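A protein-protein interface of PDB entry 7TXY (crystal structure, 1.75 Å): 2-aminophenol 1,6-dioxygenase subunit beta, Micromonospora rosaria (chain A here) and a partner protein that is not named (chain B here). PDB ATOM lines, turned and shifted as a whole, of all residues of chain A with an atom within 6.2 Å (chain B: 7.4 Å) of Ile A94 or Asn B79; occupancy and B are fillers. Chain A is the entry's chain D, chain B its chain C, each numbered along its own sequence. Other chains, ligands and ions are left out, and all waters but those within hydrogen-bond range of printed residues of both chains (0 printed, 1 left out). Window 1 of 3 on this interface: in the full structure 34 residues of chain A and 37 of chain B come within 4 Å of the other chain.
Ile A94 touches just one residue of chain B: Asn B79 (2.9 Å).
Of chain A, only Ile A94 (2.9 Å), Thr A95 (3.0 Å), Met A96 (2.8 Å) and His A100 (3.9 Å) come within 4 Å of Asn B79.
Printed residues of chain B within 4 Å of Thr A95: Asn B79.
Printed residues of chain A within 4 Å of Tyr B81: His A100 and Arg A148.
Of the printed residues of chain A, Trp B80 touches Met A96 (3.2 Å) and Val A97 (3.99 Å).
Of the printed residues of chain B, Arg A148 touches Tyr B81 (3.2 Å), Ala B82 (3.3 Å), Tyr B83 (3.3 Å) and Trp B190 (3.4 Å).
Printed residues of chain A within 4 Å of Trp B190: Val A97 (3.2 Å), His A100 (3.5 Å) and Arg A148 (3.4 Å).
Pro B17 touches none of the printed residues of chain A.
Ala A181 touches none of the printed residues of chain B.
The nearest residue of chain B that does not touch Ile A94 is Phe B58 (6.0 Å).
The nearest residue of chain A that does not touch Asn B79 is Val A97 (4.1 Å).
The backbone carbonyl oxygen (O) of Ala A181 sits at hydrogen-bond distance from the backbone NH (N) of Thr A95 (3.1 Å).
The backbone NH of Asn B79 lies within hydrogen-bond range of the side-chain carboxylate of Asp B77 (2.7 Å).
OG1 of Thr A95 lies close to OG of Ser A180 (3.2 Å).
The backbone carbonyl oxygen of Trp A93 sits at hydrogen-bond distance from the backbone NH of Ala A181.
OD1 of Asp B77 is in hydrogen-bond range of N of Trp B80, 2.9 Å away.
The backbone carbonyl oxygen (O) of Thr A95 lies within hydrogen-bond range of the backbone NH (N) of Asn A183.
Among the printed residues, pairs that only touch across the chains: Thr A95 with Asn B79 (3.0 Å), Met A96 with Leu B186 (2.9 Å), Val A97 with Trp B80 (3.99 Å), Val A97 with Leu B186 (3.8 Å), Val A97 with Trp B190 (3.2 Å), His A100 with Asn B79 (3.9 Å), His A100 with Trp B190 (3.5 Å), Arg A148 with Tyr B81 (3.2 Å), Arg A148 with Ala B82 (3.3 Å) and Arg A148 with Trp B190 (3.4 Å).
Printed residues of chain A that touch a printed residue of chain B: Trp A93, Ile A94, Thr A95, Met A96, Val A97, His A100 and Arg A148.
Along chain A the printed residues that touch a printed residue of chain B span positions 93 to 148.
Of the 16 printed residues of chain B, 8 touch a printed residue of chain A.
Hydrophobic or aromatic side chains of chain B that line the printed part of chain A: Trp B80, Tyr B81, Ala B82, Tyr B83, Leu B186 and Trp B190.
OH of Tyr B81 lies within hydrogen-bond range of ND1 of His A100 (2.8 Å).
The side-chain amide nitrogen (ND2) of Asn B79 lies within hydrogen-bond range of the backbone carbonyl oxygen (O) of Ile A94, 2.9 Å away.
The backbone NH (N) of Met A96 sits at hydrogen-bond distance from the side-chain amide oxygen (OD1) of Asn B79, at 2.8 Å.
The indole nitrogen (NE1) of Trp A93 lies within hydrogen-bond range of the backbone carbonyl oxygen (O) of Glu B78.
The indole nitrogen (NE1) of Trp B80 lies close to the side-chain sulfur (SD) of Met A96 (3.7 Å).
The guanidinium group (NH2) of Arg A148 is in hydrogen-bond range of the side-chain hydroxyl (OH) of Tyr B83 (3.3 Å).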
ATOM      1  N   ALA A  90       9.780  10.981  35.735  1.00  0.00           N
ATOM      2  CA  ALA A  90       8.532  11.007  36.483  1.00  0.00           C
ATOM      3  C   ALA A  90       7.530  10.078  35.819  1.00  0.00           C
ATOM      4  O   ALA A  90       7.655   9.771  34.628  1.00  0.00           O
ATOM      5  CB  ALA A  90       7.960  12.428  36.566  1.00  0.00           C
ATOM      6  N   PRO A  91       6.504   9.633  36.560  1.00  0.00           N
ATOM      7  CA  PRO A  91       5.645   8.557  36.051  1.00  0.00           C
ATOM      8  C   PRO A  91       4.505   8.974  35.133  1.00  0.00           C
ATOM      9  O   PRO A  91       4.060   8.165  34.314  1.00  0.00           O
ATOM     10  CB  PRO A  91       5.062   7.925  37.331  1.00  0.00           C
ATOM     11  CG  PRO A  91       5.510   8.772  38.484  1.00  0.00           C
ATOM     12  CD  PRO A  91       6.205   9.988  37.958  1.00  0.00           C
ATOM     13  N   HIS A  92       4.010  10.204  35.254  1.00  0.00           N
ATOM     14  CA  HIS A  92       2.701  10.510  34.680  1.00  0.00           C
ATOM     15  C   HIS A  92       2.739  10.846  33.196  1.00  0.00           C
ATOM     16  O   HIS A  92       1.696  10.756  32.540  1.00  0.00           O
ATOM     17  CB  HIS A  92       2.052  11.641  35.467  1.00  0.00           C
ATOM     18  CG  HIS A  92       1.696  11.248  36.869  1.00  0.00           C
ATOM     19  ND1 HIS A  92       0.674  10.369  37.153  1.00  0.00           N
ATOM     20  CD2 HIS A  92       2.254  11.576  38.058  1.00  0.00           C
ATOM     21  CE1 HIS A  92       0.598  10.194  38.460  1.00  0.00           C
ATOM     22  NE2 HIS A  92       1.543  10.918  39.032  1.00  0.00           N
ATOM     23  N   TRP A  93       3.894  11.227  32.651  1.00  0.00           N
ATOM     24  CA  TRP A  93       4.049  11.268  31.199  1.00  0.00           C
ATOM     25  C   TRP A  93       4.152   9.821  30.735  1.00  0.00           C
ATOM     26  O   TRP A  93       5.238   9.352  30.384  1.00  0.00           O
ATOM     27  CB  TRP A  93       5.269  12.090  30.797  1.00  0.00           C
ATOM     28  CG  TRP A  93       5.517  12.151  29.309  1.00  0.00           C
ATOM     29  CD1 TRP A  93       4.676  11.740  28.314  1.00  0.00           C
ATOM     30  CD2 TRP A  93       6.690  12.660  28.656  1.00  0.00           C
ATOM     31  NE1 TRP A  93       5.255  11.955  27.083  1.00  0.00           N
ATOM     32  CE2 TRP A  93       6.489  12.519  27.266  1.00  0.00           C
ATOM     33  CE3 TRP A  93       7.889  13.214  29.110  1.00  0.00           C
ATOM     34  CZ2 TRP A  93       7.443  12.915  26.332  1.00  0.00           C
ATOM     35  CZ3 TRP A  93       8.833  13.609  28.178  1.00  0.00           C
ATOM     36  CH2 TRP A  93       8.605  13.457  26.807  1.00  0.00           C
ATOM     37  N   ILE A  94       3.033   9.098  30.768  1.00  0.00           N
ATOM     38  CA  ILE A  94       3.009   7.664  30.480  1.00  0.00           C
ATOM     39  C   ILE A  94       3.028   7.506  28.962  1.00  0.00           C
ATOM     40  O   ILE A  94       2.013   7.703  28.292  1.00  0.00           O
ATOM     41  CB  ILE A  94       1.793   6.972  31.103  1.00  0.00           C
ATOM     42  CG1 ILE A  94       1.896   6.990  32.630  1.00  0.00           C
ATOM     43  CG2 ILE A  94       1.679   5.540  30.589  1.00  0.00           C
ATOM     44  CD1 ILE A  94       0.675   6.441  33.337  1.00  0.00           C
ATOM     45  N   THR A  95       4.185   7.140  28.417  1.00  0.00           N
ATOM     46  CA  THR A  95       4.348   6.919  26.987  1.00  0.00           C
ATOM     47  C   THR A  95       4.237   5.428  26.703  1.00  0.00           C
ATOM     48  O   THR A  95       5.027   4.625  27.215  1.00  0.00           O
ATOM     49  CB  THR A  95       5.683   7.470  26.492  1.00  0.00           C
ATOM     50  OG1 THR A  95       6.728   6.531  26.779  1.00  0.00           O
ATOM     51  CG2 THR A  95       5.976   8.799  27.157  1.00  0.00           C
ATOM     52  N   MET A  96       3.267   5.067  25.879  1.00  0.00           N
ATOM     53  CA  MET A  96       2.888   3.678  25.688  1.00  0.00           C
ATOM     54  C   MET A  96       3.780   2.935  24.703  1.00  0.00           C
ATOM     55  O   MET A  96       3.597   1.726  24.525  1.00  0.00           O
ATOM     56  CB  MET A  96       1.426   3.624  25.234  1.00  0.00           C
ATOM     57  CG  MET A  96       1.180   4.180  23.842  1.00  0.00           C
ATOM     58  SD  MET A  96      -0.579   4.342  23.471  1.00  0.00           S
ATOM     59  CE  MET A  96      -0.863   6.064  23.887  1.00  0.00           C
ATOM     60  N   VAL A  97       4.745   3.605  24.078  1.00  0.00           N
ATOM     61  CA  VAL A  97       5.698   2.960  23.177  1.00  0.00           C
ATOM     62  C   VAL A  97       7.087   3.435  23.600  1.00  0.00           C
ATOM     63  O   VAL A  97       7.581   4.464  23.128  1.00  0.00           O
ATOM     64  CB  VAL A  97       5.429   3.275  21.702  1.00  0.00           C
ATOM     65  CG1 VAL A  97       6.496   2.641  20.817  1.00  0.00           C
ATOM     66  CG2 VAL A  97       4.046   2.787  21.301  1.00  0.00           C
ATOM     67  N   HIS A 100      10.617   8.221  26.039  1.00  0.00           N
ATOM     68  CA  HIS A 100      10.710   9.469  25.305  1.00  0.00           C
ATOM     69  C   HIS A 100      11.585  10.457  26.060  1.00  0.00           C
ATOM     70  O   HIS A 100      11.634  10.455  27.296  1.00  0.00           O
ATOM     71  CB  HIS A 100       9.321  10.075  25.064  1.00  0.00           C
ATOM     72  CG  HIS A 100       8.405   9.193  24.269  1.00  0.00           C
ATOM     73  ND1 HIS A 100       7.470   9.696  23.388  1.00  0.00           N
ATOM     74  CD2 HIS A 100       8.273   7.847  24.229  1.00  0.00           C
ATOM     75  CE1 HIS A 100       6.806   8.696  22.837  1.00  0.00           C
ATOM     76  NE2 HIS A 100       7.275   7.563  23.328  1.00  0.00           N
ATOM     77  N   ARG A 148      12.265   7.693  21.527  1.00  0.00           N
ATOM     78  CA  ARG A 148      11.846   8.757  20.626  1.00  0.00           C
ATOM     79  C   ARG A 148      12.220  10.088  21.256  1.00  0.00           C
ATOM     80  O   ARG A 148      12.138  10.243  22.478  1.00  0.00           O
ATOM     81  CB  ARG A 148      10.341   8.716  20.342  1.00  0.00           C
ATOM     82  CG  ARG A 148       9.884   9.777  19.345  1.00  0.00           C
ATOM     83  CD  ARG A 148       8.396   9.675  19.039  1.00  0.00           C
ATOM     84  NE  ARG A 148       8.088   8.537  18.178  1.00  0.00           N
ATOM     85  CZ  ARG A 148       8.304   8.502  16.871  1.00  0.00           C
ATOM     86  NH1 ARG A 148       8.839   9.529  16.230  1.00  0.00           N
ATOM     87  NH2 ARG A 148       7.976   7.408  16.189  1.00  0.00           N
ATOM     88  N   SER A 180      10.501  10.507  29.966  1.00  0.00           N
ATOM     89  CA  SER A 180       9.152   9.981  30.072  1.00  0.00           C
ATOM     90  C   SER A 180       9.158   8.597  30.713  1.00  0.00           C
ATOM     91  O   SER A 180      10.204   7.964  30.887  1.00  0.00           O
ATOM     92  CB  SER A 180       8.508   9.920  28.689  1.00  0.00           C
ATOM     93  OG  SER A 180       8.780   8.675  28.059  1.00  0.00           O
ATOM     94  N   ALA A 181       7.962   8.119  31.051  1.00  0.00           N
ATOM     95  CA  ALA A 181       7.780   6.888  31.812  1.00  0.00           C
ATOM     96  C   ALA A 181       7.086   5.849  30.943  1.00  0.00           C
ATOM     97  O   ALA A 181       5.891   5.965  30.659  1.00  0.00           O
ATOM     98  CB  ALA A 181       6.974   7.151  33.084  1.00  0.00           C
ATOM     99  N   ASN A 182       7.831   4.819  30.551  1.00  0.00           N
ATOM    100  CA  ASN A 182       7.252   3.720  29.790  1.00  0.00           C
ATOM    101  C   ASN A 182       6.250   2.961  30.655  1.00  0.00           C
ATOM    102  O   ASN A 182       6.620   2.368  31.675  1.00  0.00           O
ATOM    103  CB  ASN A 182       8.352   2.782  29.297  1.00  0.00           C
ATOM    104  CG  ASN A 182       7.802   1.561  28.586  1.00  0.00           C
ATOM    105  OD1 ASN A 182       8.117   0.428  28.938  1.00  0.00           O
ATOM    106  ND2 ASN A 182       6.969   1.792  27.574  1.00  0.00           N
ATOM    107  N   ASN A 183       4.986   2.985  30.250  1.00  0.00           N
ATOM    108  CA  ASN A 183       3.933   2.236  30.922  1.00  0.00           C
ATOM    109  C   ASN A 183       2.745   2.157  29.971  1.00  0.00           C
ATOM    110  O   ASN A 183       2.792   2.663  28.846  1.00  0.00           O
ATOM    111  CB  ASN A 183       3.549   2.882  32.257  1.00  0.00           C
ATOM    112  CG  ASN A 183       3.408   1.866  33.379  1.00  0.00           C
ATOM    113  OD1 ASN A 183       2.427   1.123  33.440  1.00  0.00           O
ATOM    114  ND2 ASN A 183       4.390   1.831  34.273  1.00  0.00           N
ATOM    115  N   ASN A 184       1.674   1.512  30.430  1.00  0.00           N
ATOM    116  CA  ASN A 184       0.461   1.380  29.634  1.00  0.00           C
ATOM    117  C   ASN A 184      -0.589   2.340  30.168  1.00  0.00           C
ATOM    118  O   ASN A 184      -1.033   2.172  31.315  1.00  0.00           O
ATOM    119  CB  ASN A 184      -0.055  -0.055  29.681  1.00  0.00           C
ATOM    120  CG  ASN A 184      -1.172  -0.311  28.683  1.00  0.00           C
ATOM    121  OD1 ASN A 184      -1.769   0.622  28.146  1.00  0.00           O
ATOM    122  ND2 ASN A 184      -1.456  -1.584  28.426  1.00  0.00           N
ATOM    123  N   PRO A 185      -1.014   3.350  29.398  1.00  0.00           N
ATOM    124  CA  PRO A 185      -2.000   4.309  29.926  1.00  0.00           C
ATOM    125  C   PRO A 185      -3.395   3.727  30.100  1.00  0.00           C
ATOM    126  O   PRO A 185      -4.216   4.345  30.790  1.00  0.00           O
ATOM    127  CB  PRO A 185      -1.995   5.432  28.879  1.00  0.00           C
ATOM    128  CG  PRO A 185      -1.578   4.768  27.618  1.00  0.00           C
ATOM    129  CD  PRO A 185      -0.625   3.666  28.009  1.00  0.00           C
ATOM    130  N   TYR A 188      -2.594   0.235  33.573  1.00  0.00           N
ATOM    131  CA  TYR A 188      -1.371   0.579  34.283  1.00  0.00           C
ATOM    132  C   TYR A 188      -0.801  -0.646  34.987  1.00  0.00           C
ATOM    133  O   TYR A 188      -1.532  -1.434  35.596  1.00  0.00           O
ATOM    134  CB  TYR A 188      -1.644   1.696  35.289  1.00  0.00           C
ATOM    135  CG  TYR A 188      -0.386   2.338  35.827  1.00  0.00           C
ATOM    136  CD1 TYR A 188       0.433   3.104  35.008  1.00  0.00           C
ATOM    137  CD2 TYR A 188      -0.020   2.183  37.155  1.00  0.00           C
ATOM    138  CE1 TYR A 188       1.582   3.689  35.493  1.00  0.00           C
ATOM    139  CE2 TYR A 188       1.123   2.767  37.650  1.00  0.00           C
ATOM    140  CZ  TYR A 188       1.924   3.516  36.817  1.00  0.00           C
ATOM    141  OH  TYR A 188       3.070   4.094  37.313  1.00  0.00           O
ATOM    142  N   PRO B  17      -6.189   8.031  18.855  1.00  0.00           N
ATOM    143  CA  PRO B  17      -6.210   8.976  17.732  1.00  0.00           C
ATOM    144  C   PRO B  17      -5.946   8.325  16.388  1.00  0.00           C
ATOM    145  O   PRO B  17      -6.118   8.994  15.360  1.00  0.00           O
ATOM    146  CB  PRO B  17      -5.104   9.972  18.089  1.00  0.00           C
ATOM    147  CG  PRO B  17      -4.159   9.199  18.937  1.00  0.00           C
ATOM    148  CD  PRO B  17      -4.991   8.197  19.703  1.00  0.00           C
ATOM    149  N   HIS B  18      -5.554   7.054  16.369  1.00  0.00           N
ATOM    150  CA  HIS B  18      -5.293   6.361  15.111  1.00  0.00           C
ATOM    151  C   HIS B  18      -6.528   6.300  14.220  1.00  0.00           C
ATOM    152  O   HIS B  18      -6.394   6.100  13.006  1.00  0.00           O
ATOM    153  CB  HIS B  18      -4.784   4.951  15.396  1.00  0.00           C
ATOM    154  CG  HIS B  18      -3.593   4.907  16.300  1.00  0.00           C
ATOM    155  ND1 HIS B  18      -3.663   5.225  17.640  1.00  0.00           N
ATOM    156  CD2 HIS B  18      -2.300   4.589  16.056  1.00  0.00           C
ATOM    157  CE1 HIS B  18      -2.465   5.100  18.181  1.00  0.00           C
ATOM    158  NE2 HIS B  18      -1.619   4.719  17.242  1.00  0.00           N
ATOM    159  N   PHE B  58      -9.293  10.120  33.425  1.00  0.00           N
ATOM    160  CA  PHE B  58      -9.400   9.306  34.622  1.00  0.00           C
ATOM    161  C   PHE B  58      -9.210  10.170  35.862  1.00  0.00           C
ATOM    162  O   PHE B  58      -8.698  11.290  35.800  1.00  0.00           O
ATOM    163  CB  PHE B  58      -8.364   8.181  34.606  1.00  0.00           C
ATOM    164  CG  PHE B  58      -6.944   8.666  34.547  1.00  0.00           C
ATOM    165  CD1 PHE B  58      -6.261   8.989  35.707  1.00  0.00           C
ATOM    166  CD2 PHE B  58      -6.291   8.789  33.336  1.00  0.00           C
ATOM    167  CE1 PHE B  58      -4.953   9.432  35.658  1.00  0.00           C
ATOM    168  CE2 PHE B  58      -4.983   9.235  33.278  1.00  0.00           C
ATOM    169  CZ  PHE B  58      -4.315   9.555  34.443  1.00  0.00           C
ATOM    170  N   VAL B  76      -1.975  18.442  21.136  1.00  0.00           N
ATOM    171  CA  VAL B  76      -0.968  17.565  20.557  1.00  0.00           C
ATOM    172  C   VAL B  76      -0.741  16.421  21.538  1.00  0.00           C
ATOM    173  O   VAL B  76      -0.229  16.628  22.645  1.00  0.00           O
ATOM    174  CB  VAL B  76       0.337  18.313  20.254  1.00  0.00           C
ATOM    175  CG1 VAL B  76       1.362  17.368  19.629  1.00  0.00           C
ATOM    176  CG2 VAL B  76       0.060  19.493  19.335  1.00  0.00           C
ATOM    177  N   ASP B  77      -1.125  15.215  21.129  1.00  0.00           N
ATOM    178  CA  ASP B  77      -1.039  14.054  22.003  1.00  0.00           C
ATOM    179  C   ASP B  77       0.395  13.824  22.456  1.00  0.00           C
ATOM    180  O   ASP B  77       1.337  13.891  21.660  1.00  0.00           O
ATOM    181  CB  ASP B  77      -1.573  12.818  21.280  1.00  0.00           C
ATOM    182  CG  ASP B  77      -1.686  11.614  22.186  1.00  0.00           C
ATOM    183  OD1 ASP B  77      -0.695  10.866  22.300  1.00  0.00           O
ATOM    184  OD2 ASP B  77      -2.772  11.414  22.780  1.00  0.00           O
ATOM    185  N   GLU B  78       0.552  13.538  23.752  1.00  0.00           N
ATOM    186  CA  GLU B  78       1.863  13.356  24.359  1.00  0.00           C
ATOM    187  C   GLU B  78       2.541  12.058  23.946  1.00  0.00           C
ATOM    188  O   GLU B  78       3.723  11.875  24.259  1.00  0.00           O
ATOM    189  CB  GLU B  78       1.726  13.386  25.887  1.00  0.00           C
ATOM    190  CG  GLU B  78       1.403  14.754  26.472  1.00  0.00           C
ATOM    191  CD  GLU B  78      -0.091  15.062  26.479  1.00  0.00           C
ATOM    192  OE1 GLU B  78      -0.461  16.199  26.863  1.00  0.00           O
ATOM    193  OE2 GLU B  78      -0.893  14.187  26.076  1.00  0.00           O
ATOM    194  N   ASN B  79       1.827  11.156  23.279  1.00  0.00           N
ATOM    195  CA  ASN B  79       2.361   9.885  22.810  1.00  0.00           C
ATOM    196  C   ASN B  79       2.519   9.818  21.298  1.00  0.00           C
ATOM    197  O   ASN B  79       3.479   9.221  20.810  1.00  0.00           O
ATOM    198  CB  ASN B  79       1.444   8.740  23.251  1.00  0.00           C
ATOM    199  CG  ASN B  79       2.035   7.916  24.365  1.00  0.00           C
ATOM    200  OD1 ASN B  79       3.136   7.380  24.234  1.00  0.00           O
ATOM    201  ND2 ASN B  79       1.304   7.801  25.470  1.00  0.00           N
ATOM    202  N   TRP B  80       1.589  10.411  20.547  1.00  0.00           N
ATOM    203  CA  TRP B  80       1.545  10.292  19.094  1.00  0.00           C
ATOM    204  C   TRP B  80       1.815  11.618  18.394  1.00  0.00           C
ATOM    205  O   TRP B  80       1.434  11.791  17.232  1.00  0.00           O
ATOM    206  CB  TRP B  80       0.191   9.722  18.674  1.00  0.00           C
ATOM    207  CG  TRP B  80      -0.090   8.434  19.365  1.00  0.00           C
ATOM    208  CD1 TRP B  80      -0.938   8.231  20.410  1.00  0.00           C
ATOM    209  CD2 TRP B  80       0.502   7.163  19.076  1.00  0.00           C
ATOM    210  NE1 TRP B  80      -0.918   6.914  20.790  1.00  0.00           N
ATOM    211  CE2 TRP B  80      -0.040   6.235  19.986  1.00  0.00           C
ATOM    212  CE3 TRP B  80       1.433   6.721  18.135  1.00  0.00           C
ATOM    213  CZ2 TRP B  80       0.315   4.891  19.979  1.00  0.00           C
ATOM    214  CZ3 TRP B  80       1.788   5.384  18.131  1.00  0.00           C
ATOM    215  CH2 TRP B  80       1.230   4.486  19.047  1.00  0.00           C
ATOM    216  N   TYR B  81       2.498  12.542  19.077  1.00  0.00           N
ATOM    217  CA  TYR B  81       2.809  13.842  18.502  1.00  0.00           C
ATOM    218  C   TYR B  81       3.516  13.728  17.159  1.00  0.00           C
ATOM    219  O   TYR B  81       3.367  14.606  16.304  1.00  0.00           O
ATOM    220  CB  TYR B  81       3.681  14.640  19.480  1.00  0.00           C
ATOM    221  CG  TYR B  81       4.869  13.864  20.026  1.00  0.00           C
ATOM    222  CD1 TYR B  81       6.051  13.766  19.307  1.00  0.00           C
ATOM    223  CD2 TYR B  81       4.803  13.232  21.263  1.00  0.00           C
ATOM    224  CE1 TYR B  81       7.133  13.058  19.794  1.00  0.00           C
ATOM    225  CE2 TYR B  81       5.885  12.518  21.766  1.00  0.00           C
ATOM    226  CZ  TYR B  81       7.048  12.438  21.029  1.00  0.00           C
ATOM    227  OH  TYR B  81       8.128  11.733  21.518  1.00  0.00           O
ATOM    228  N   ALA B  82       4.289  12.661  16.954  1.00  0.00           N
ATOM    229  CA  ALA B  82       5.083  12.530  15.737  1.00  0.00           C
ATOM    230  C   ALA B  82       4.251  12.161  14.516  1.00  0.00           C
ATOM    231  O   ALA B  82       4.761  12.254  13.392  1.00  0.00           O
ATOM    232  CB  ALA B  82       6.180  11.483  15.944  1.00  0.00           C
ATOM    233  N   TYR B  83       2.998  11.759  14.701  1.00  0.00           N
ATOM    234  CA  TYR B  83       2.127  11.334  13.618  1.00  0.00           C
ATOM    235  C   TYR B  83       1.071  12.396  13.352  1.00  0.00           C
ATOM    236  O   TYR B  83       0.761  13.230  14.207  1.00  0.00           O
ATOM    237  CB  TYR B  83       1.464   9.993  13.950  1.00  0.00           C
ATOM    238  CG  TYR B  83       2.458   8.906  14.299  1.00  0.00           C
ATOM    239  CD1 TYR B  83       3.013   8.823  15.569  1.00  0.00           C
ATOM    240  CD2 TYR B  83       2.853   7.974  13.351  1.00  0.00           C
ATOM    241  CE1 TYR B  83       3.928   7.835  15.887  1.00  0.00           C
ATOM    242  CE2 TYR B  83       3.762   6.983  13.659  1.00  0.00           C
ATOM    243  CZ  TYR B  83       4.298   6.916  14.926  1.00  0.00           C
ATOM    244  OH  TYR B  83       5.209   5.931  15.233  1.00  0.00           O
ATOM    245  N   TYR B  85      -2.082  12.195  13.141  1.00  0.00           N
ATOM    246  CA  TYR B  85      -3.240  12.090  14.019  1.00  0.00           C
ATOM    247  C   TYR B  85      -2.923  12.464  15.463  1.00  0.00           C
ATOM    248  O   TYR B  85      -3.827  12.426  16.303  1.00  0.00           O
ATOM    249  CB  TYR B  85      -3.821  10.670  13.960  1.00  0.00           C
ATOM    250  CG  TYR B  85      -2.816   9.550  14.127  1.00  0.00           C
ATOM    251  CD1 TYR B  85      -2.447   9.101  15.382  1.00  0.00           C
ATOM    252  CD2 TYR B  85      -2.252   8.925  13.018  1.00  0.00           C
ATOM    253  CE1 TYR B  85      -1.542   8.077  15.541  1.00  0.00           C
ATOM    254  CE2 TYR B  85      -1.339   7.895  13.165  1.00  0.00           C
ATOM    255  CZ  TYR B  85      -0.990   7.473  14.428  1.00  0.00           C
ATOM    256  OH  TYR B  85      -0.088   6.446  14.583  1.00  0.00           O
ATOM    257  N   GLY B  86      -1.671  12.816  15.766  1.00  0.00           N
ATOM    258  CA  GLY B  86      -1.347  13.363  17.069  1.00  0.00           C
ATOM    259  C   GLY B  86      -1.735  14.813  17.249  1.00  0.00           C
ATOM    260  O   GLY B  86      -1.873  15.269  18.389  1.00  0.00           O
ATOM    261  N   THR B 125      -7.609  12.885  24.834  1.00  0.00           N
ATOM    262  CA  THR B 125      -7.611  12.563  23.408  1.00  0.00           C
ATOM    263  C   THR B 125      -8.838  11.753  23.017  1.00  0.00           C
ATOM    264  O   THR B 125      -9.379  11.923  21.914  1.00  0.00           O
ATOM    265  CB  THR B 125      -6.332  11.799  23.058  1.00  0.00           C
ATOM    266  OG1 THR B 125      -5.212  12.680  23.222  1.00  0.00           O
ATOM    267  CG2 THR B 125      -6.375  11.273  21.618  1.00  0.00           C
ATOM    268  N   LEU B 186      -0.800  -3.368  24.096  1.00  0.00           N
ATOM    269  CA  LEU B 186      -0.227  -2.488  23.093  1.00  0.00           C
ATOM    270  C   LEU B 186       1.103  -3.028  22.578  1.00  0.00           C
ATOM    271  O   LEU B 186       1.892  -3.607  23.329  1.00  0.00           O
ATOM    272  CB  LEU B 186      -0.022  -1.090  23.665  1.00  0.00           C
ATOM    273  CG  LEU B 186       0.193  -0.049  22.568  1.00  0.00           C
ATOM    274  CD1 LEU B 186      -1.109   0.647  22.215  1.00  0.00           C
ATOM    275  CD2 LEU B 186       1.244   0.946  22.989  1.00  0.00           C
ATOM    276  N   TRP B 190       7.581   0.945  17.332  1.00  0.00           N
ATOM    277  CA  TRP B 190       7.183   1.932  16.328  1.00  0.00           C
ATOM    278  C   TRP B 190       6.930   1.192  15.021  1.00  0.00           C
ATOM    279  O   TRP B 190       7.800   1.093  14.156  1.00  0.00           O
ATOM    280  CB  TRP B 190       8.249   3.009  16.171  1.00  0.00           C
ATOM    281  CG  TRP B 190       8.538   3.751  17.438  1.00  0.00           C
ATOM    282  CD1 TRP B 190       9.718   3.772  18.122  1.00  0.00           C
ATOM    283  CD2 TRP B 190       7.631   4.579  18.178  1.00  0.00           C
ATOM    284  NE1 TRP B 190       9.603   4.563  19.239  1.00  0.00           N
ATOM    285  CE2 TRP B 190       8.330   5.069  19.299  1.00  0.00           C
ATOM    286  CE3 TRP B 190       6.295   4.952  18.005  1.00  0.00           C
ATOM    287  CZ2 TRP B 190       7.741   5.911  20.236  1.00  0.00           C
ATOM    288  CZ3 TRP B 190       5.712   5.788  18.937  1.00  0.00           C
ATOM    289  CH2 TRP B 190       6.433   6.258  20.038  1.00  0.00           C
